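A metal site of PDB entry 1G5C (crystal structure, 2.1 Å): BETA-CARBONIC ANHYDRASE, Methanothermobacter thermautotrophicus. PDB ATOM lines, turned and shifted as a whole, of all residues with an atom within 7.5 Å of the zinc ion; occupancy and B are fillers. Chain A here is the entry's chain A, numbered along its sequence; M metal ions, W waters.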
ATOM      1  N   THR A  31      -2.466  11.265 -21.691  1.00  0.00           N
ATOM      2  CA  THR A  31      -3.400  10.187 -21.446  1.00  0.00           C
ATOM      3  C   THR A  31      -3.066   9.368 -20.197  1.00  0.00           C
ATOM      4  O   THR A  31      -2.231   9.792 -19.373  1.00  0.00           O
ATOM      5  CB  THR A  31      -3.530   9.279 -22.717  1.00  0.00           C
ATOM      6  OG1 THR A  31      -4.647   8.380 -22.562  1.00  0.00           O
ATOM      7  CG2 THR A  31      -2.213   8.483 -22.969  1.00  0.00           C
ATOM      8  N   CYS A  32      -3.710   8.218 -20.046  1.00  0.00           N
ATOM      9  CA  CYS A  32      -3.521   7.400 -18.846  1.00  0.00           C
ATOM     10  C   CYS A  32      -2.476   6.304 -19.016  1.00  0.00           C
ATOM     11  O   CYS A  32      -2.112   5.942 -20.133  1.00  0.00           O
ATOM     12  CB  CYS A  32      -4.876   6.788 -18.427  1.00  0.00           C
ATOM     13  SG  CYS A  32      -4.853   5.861 -16.864  1.00  0.00           S
ATOM     14  N   MET A  33      -2.028   5.737 -17.883  1.00  0.00           N
ATOM     15  CA  MET A  33      -1.015   4.682 -17.886  1.00  0.00           C
ATOM     16  C   MET A  33      -1.603   3.283 -18.135  1.00  0.00           C
ATOM     17  O   MET A  33      -0.857   2.290 -18.232  1.00  0.00           O
ATOM     18  CB  MET A  33      -0.254   4.700 -16.543  1.00  0.00           C
ATOM     19  CG  MET A  33      -1.113   4.262 -15.374  1.00  0.00           C
ATOM     20  SD  MET A  33      -0.320   4.481 -13.779  1.00  0.00           S
ATOM     21  CE  MET A  33       0.637   3.084 -13.671  1.00  0.00           C
ATOM     22  N   ASP A  34      -2.928   3.236 -18.245  1.00  0.00           N
ATOM     23  CA  ASP A  34      -3.671   1.996 -18.490  1.00  0.00           C
ATOM     24  C   ASP A  34      -3.031   1.158 -19.608  1.00  0.00           C
ATOM     25  O   ASP A  34      -2.773   1.650 -20.711  1.00  0.00           O
ATOM     26  CB  ASP A  34      -5.138   2.338 -18.875  1.00  0.00           C
ATOM     27  CG  ASP A  34      -6.071   1.149 -18.666  1.00  0.00           C
ATOM     28  OD1 ASP A  34      -6.017   0.193 -19.463  1.00  0.00           O
ATOM     29  OD2 ASP A  34      -6.838   1.168 -17.682  1.00  0.00           O
ATOM     30  N   SER A  35      -2.792  -0.119 -19.325  1.00  0.00           N
ATOM     31  CA  SER A  35      -2.151  -1.003 -20.300  1.00  0.00           C
ATOM     32  C   SER A  35      -2.945  -1.282 -21.566  1.00  0.00           C
ATOM     33  O   SER A  35      -2.356  -1.671 -22.583  1.00  0.00           O
ATOM     34  CB  SER A  35      -1.773  -2.358 -19.662  1.00  0.00           C
ATOM     35  OG  SER A  35      -2.917  -3.155 -19.437  1.00  0.00           O
ATOM     36  N   ARG A  36      -4.254  -1.059 -21.532  1.00  0.00           N
ATOM     37  CA  ARG A  36      -5.066  -1.307 -22.720  1.00  0.00           C
ATOM     38  C   ARG A  36      -4.944  -0.216 -23.773  1.00  0.00           C
ATOM     39  O   ARG A  36      -5.449  -0.356 -24.895  1.00  0.00           O
ATOM     40  CB  ARG A  36      -6.531  -1.476 -22.307  1.00  0.00           C
ATOM     41  CG  ARG A  36      -6.753  -2.695 -21.438  1.00  0.00           C
ATOM     42  CD  ARG A  36      -8.124  -2.678 -20.850  1.00  0.00           C
ATOM     43  NE  ARG A  36      -8.204  -1.677 -19.786  1.00  0.00           N
ATOM     44  CZ  ARG A  36      -9.317  -1.412 -19.110  1.00  0.00           C
ATOM     45  NH1 ARG A  36     -10.457  -2.043 -19.376  1.00  0.00           N
ATOM     46  NH2 ARG A  36      -9.261  -0.506 -18.142  1.00  0.00           N
ATOM     47  N   LEU A  37      -4.266   0.876 -23.418  1.00  0.00           N
ATOM     48  CA  LEU A  37      -4.072   1.968 -24.362  1.00  0.00           C
ATOM     49  C   LEU A  37      -2.823   1.732 -25.203  1.00  0.00           C
ATOM     50  O   LEU A  37      -2.636   2.371 -26.241  1.00  0.00           O
ATOM     51  CB  LEU A  37      -3.933   3.306 -23.622  1.00  0.00           C
ATOM     52  CG  LEU A  37      -5.237   3.809 -22.993  1.00  0.00           C
ATOM     53  CD1 LEU A  37      -4.966   4.966 -22.031  1.00  0.00           C
ATOM     54  CD2 LEU A  37      -6.193   4.229 -24.115  1.00  0.00           C
ATOM     55  N   ASN A  57       0.063   9.381 -16.955  1.00  0.00           N
ATOM     56  CA  ASN A  57       0.096   9.208 -15.509  1.00  0.00           C
ATOM     57  C   ASN A  57      -1.200   8.489 -15.135  1.00  0.00           C
ATOM     58  O   ASN A  57      -1.966   8.108 -16.031  1.00  0.00           O
ATOM     59  CB  ASN A  57       0.217  10.567 -14.794  1.00  0.00           C
ATOM     60  CG  ASN A  57      -1.021  11.472 -14.976  1.00  0.00           C
ATOM     61  OD1 ASN A  57      -2.066  11.059 -15.484  1.00  0.00           O
ATOM     62  ND2 ASN A  57      -0.893  12.703 -14.521  1.00  0.00           N
ATOM     63  N   ALA A  58      -1.453   8.274 -13.853  1.00  0.00           N
ATOM     64  CA  ALA A  58      -2.653   7.550 -13.468  1.00  0.00           C
ATOM     65  C   ALA A  58      -3.923   8.387 -13.620  1.00  0.00           C
ATOM     66  O   ALA A  58      -4.120   9.359 -12.886  1.00  0.00           O
ATOM     67  CB  ALA A  58      -2.526   7.053 -12.008  1.00  0.00           C
ATOM     68  N   GLY A  59      -4.768   8.027 -14.581  1.00  0.00           N
ATOM     69  CA  GLY A  59      -6.015   8.753 -14.800  1.00  0.00           C
ATOM     70  C   GLY A  59      -5.957   9.992 -15.665  1.00  0.00           C
ATOM     71  O   GLY A  59      -6.938  10.730 -15.753  1.00  0.00           O
ATOM     72  N   ASN A  60      -4.814  10.216 -16.332  1.00  0.00           N
ATOM     73  CA  ASN A  60      -4.607  11.393 -17.175  1.00  0.00           C
ATOM     74  C   ASN A  60      -5.125  12.660 -16.499  1.00  0.00           C
ATOM     75  O   ASN A  60      -5.905  13.440 -17.067  1.00  0.00           O
ATOM     76  CB  ASN A  60      -5.214  11.229 -18.574  1.00  0.00           C
ATOM     77  CG  ASN A  60      -6.684  10.821 -18.550  1.00  0.00           C
ATOM     78  OD1 ASN A  60      -7.015   9.644 -18.475  1.00  0.00           O
ATOM     79  ND2 ASN A  60      -7.574  11.799 -18.619  1.00  0.00           N
ATOM     80  N   VAL A  85      -6.484  12.690 -23.697  1.00  0.00           N
ATOM     81  CA  VAL A  85      -7.334  11.561 -24.078  1.00  0.00           C
ATOM     82  C   VAL A  85      -7.644  10.683 -22.852  1.00  0.00           C
ATOM     83  O   VAL A  85      -6.772   9.961 -22.324  1.00  0.00           O
ATOM     84  CB  VAL A  85      -6.675  10.665 -25.171  1.00  0.00           C
ATOM     85  CG1 VAL A  85      -7.628   9.541 -25.571  1.00  0.00           C
ATOM     86  CG2 VAL A  85      -6.324  11.514 -26.391  1.00  0.00           C
ATOM     87  N   GLY A  86      -8.873  10.781 -22.359  1.00  0.00           N
ATOM     88  CA  GLY A  86      -9.263   9.938 -21.250  1.00  0.00           C
ATOM     89  C   GLY A  86      -9.801   8.663 -21.870  1.00  0.00           C
ATOM     90  O   GLY A  86      -9.847   8.556 -23.099  1.00  0.00           O
ATOM     91  N   HIS A  87     -10.218   7.698 -21.071  1.00  0.00           N
ATOM     92  CA  HIS A  87     -10.744   6.472 -21.650  1.00  0.00           C
ATOM     93  C   HIS A  87     -11.803   5.879 -20.725  1.00  0.00           C
ATOM     94  O   HIS A  87     -11.797   6.121 -19.533  1.00  0.00           O
ATOM     95  CB  HIS A  87      -9.634   5.444 -21.865  1.00  0.00           C
ATOM     96  CG  HIS A  87      -9.024   4.943 -20.596  1.00  0.00           C
ATOM     97  ND1 HIS A  87      -9.478   3.814 -19.942  1.00  0.00           N
ATOM     98  CD2 HIS A  87      -8.038   5.451 -19.823  1.00  0.00           C
ATOM     99  CE1 HIS A  87      -8.791   3.648 -18.828  1.00  0.00           C
ATOM    100  NE2 HIS A  87      -7.905   4.619 -18.717  1.00  0.00           N
ATOM    101  N   THR A  88     -12.704   5.090 -21.312  1.00  0.00           N
ATOM    102  CA  THR A  88     -13.759   4.457 -20.531  1.00  0.00           C
ATOM    103  C   THR A  88     -13.140   3.373 -19.662  1.00  0.00           C
ATOM    104  O   THR A  88     -12.076   2.820 -19.986  1.00  0.00           O
ATOM    105  CB  THR A  88     -14.805   3.814 -21.432  1.00  0.00           C
ATOM    106  OG1 THR A  88     -14.156   2.892 -22.320  1.00  0.00           O
ATOM    107  CG2 THR A  88     -15.538   4.858 -22.270  1.00  0.00           C
ATOM    108  N   ASP A  89     -13.811   3.064 -18.562  1.00  0.00           N
ATOM    109  CA  ASP A  89     -13.372   2.059 -17.599  1.00  0.00           C
ATOM    110  C   ASP A  89     -11.989   2.361 -17.029  1.00  0.00           C
ATOM    111  O   ASP A  89     -11.125   1.488 -16.968  1.00  0.00           O
ATOM    112  CB  ASP A  89     -13.381   0.662 -18.249  1.00  0.00           C
ATOM    113  CG  ASP A  89     -13.199  -0.449 -17.212  1.00  0.00           C
ATOM    114  OD1 ASP A  89     -13.689  -0.291 -16.100  1.00  0.00           O
ATOM    115  OD2 ASP A  89     -12.579  -1.478 -17.528  1.00  0.00           O
ATOM    116  N   CYS A  90     -11.799   3.600 -16.600  1.00  0.00           N
ATOM    117  CA  CYS A  90     -10.535   4.037 -16.014  1.00  0.00           C
ATOM    118  C   CYS A  90     -10.530   3.631 -14.534  1.00  0.00           C
ATOM    119  O   CYS A  90      -9.636   2.928 -14.077  1.00  0.00           O
ATOM    120  CB  CYS A  90     -10.361   5.548 -16.154  1.00  0.00           C
ATOM    121  SG  CYS A  90      -8.772   6.168 -15.558  1.00  0.00           S
ATOM    122  N   GLY A  91     -11.544   4.045 -13.791  1.00  0.00           N
ATOM    123  CA  GLY A  91     -11.588   3.646 -12.401  1.00  0.00           C
ATOM    124  C   GLY A  91     -10.864   4.546 -11.426  1.00  0.00           C
ATOM    125  O   GLY A  91     -11.071   4.434 -10.213  1.00  0.00           O
ATOM    126  N   MET A  92     -10.010   5.435 -11.922  1.00  0.00           N
ATOM    127  CA  MET A  92      -9.328   6.366 -11.030  1.00  0.00           C
ATOM    128  C   MET A  92     -10.496   7.153 -10.447  1.00  0.00           C
ATOM    129  O   MET A  92     -10.364   7.859  -9.443  1.00  0.00           O
ATOM    130  CB  MET A  92      -8.402   7.300 -11.808  1.00  0.00           C
ATOM    131  CG  MET A  92      -7.029   6.725 -12.063  1.00  0.00           C
ATOM    132  SD  MET A  92      -6.183   6.288 -10.525  1.00  0.00           S
ATOM    133  CE  MET A  92      -5.645   7.903  -9.970  1.00  0.00           C
ATOM    134  N   GLU A 128     -14.559   9.956 -15.601  1.00  0.00           N
ATOM    135  CA  GLU A 128     -13.824  10.092 -16.863  1.00  0.00           C
ATOM    136  C   GLU A 128     -13.991  11.340 -17.735  1.00  0.00           C
ATOM    137  O   GLU A 128     -13.022  12.067 -17.956  1.00  0.00           O
ATOM    138  CB  GLU A 128     -14.013   8.828 -17.707  1.00  0.00           C
ATOM    139  CG  GLU A 128     -13.321   7.596 -17.126  1.00  0.00           C
ATOM    140  CD  GLU A 128     -14.220   6.753 -16.219  1.00  0.00           C
ATOM    141  OE1 GLU A 128     -15.207   7.295 -15.671  1.00  0.00           O
ATOM    142  OE2 GLU A 128     -13.925   5.544 -16.050  1.00  0.00           O
ATOM    143  N   ILE A 158     -12.234   2.190 -24.374  1.00  0.00           N
ATOM    144  CA  ILE A 158     -11.089   1.333 -24.130  1.00  0.00           C
ATOM    145  C   ILE A 158     -11.093  -0.026 -24.851  1.00  0.00           C
ATOM    146  O   ILE A 158     -10.046  -0.674 -25.002  1.00  0.00           O
ATOM    147  CB  ILE A 158     -10.883   1.153 -22.593  1.00  0.00           C
ATOM    148  CG1 ILE A 158      -9.459   0.634 -22.308  1.00  0.00           C
ATOM    149  CG2 ILE A 158     -11.942   0.201 -22.003  1.00  0.00           C
ATOM    150  CD1 ILE A 158      -8.345   1.584 -22.787  1.00  0.00           C
HETATM  151 ZN    ZN M   1      -7.107   5.032 -16.837  1.00  0.00          ZN
HETATM  152  O   HOH W   1      -7.153   3.093 -16.227  1.00  0.00           O
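Asp 34 touches the zinc ion.
Of the 21 residues printed, 4 come within 4 Å of the zinc ion.
The zinc ion is bound by water W1 (2.0 Å), NE2 of His 87 (2.1 Å), SG of Cys 90 (2.4 Å) and SG of Cys 32 (2.4 Å).
The zinc ion has four donor atoms within binding distance.
SG of Cys 32 sits close to N of Gly 59, at 3.1 Å.
SG of Cys 32 sits close to N of Asp 34, at 3.5 Å.
The backbone NH (N) of Cys 90 sits at hydrogen-bond distance from the side-chain carboxylate (OE2) of Glu 128 (2.9 Å).
OD1 of Asp 34 is in salt-bridge range of NE of Arg 36 (2.9 Å).
O of Asn 57 sits close to SG of Cys 32, 3.8 Å away.
Water W1 bridges OD2 of Asp 34 and O of Cys 90.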
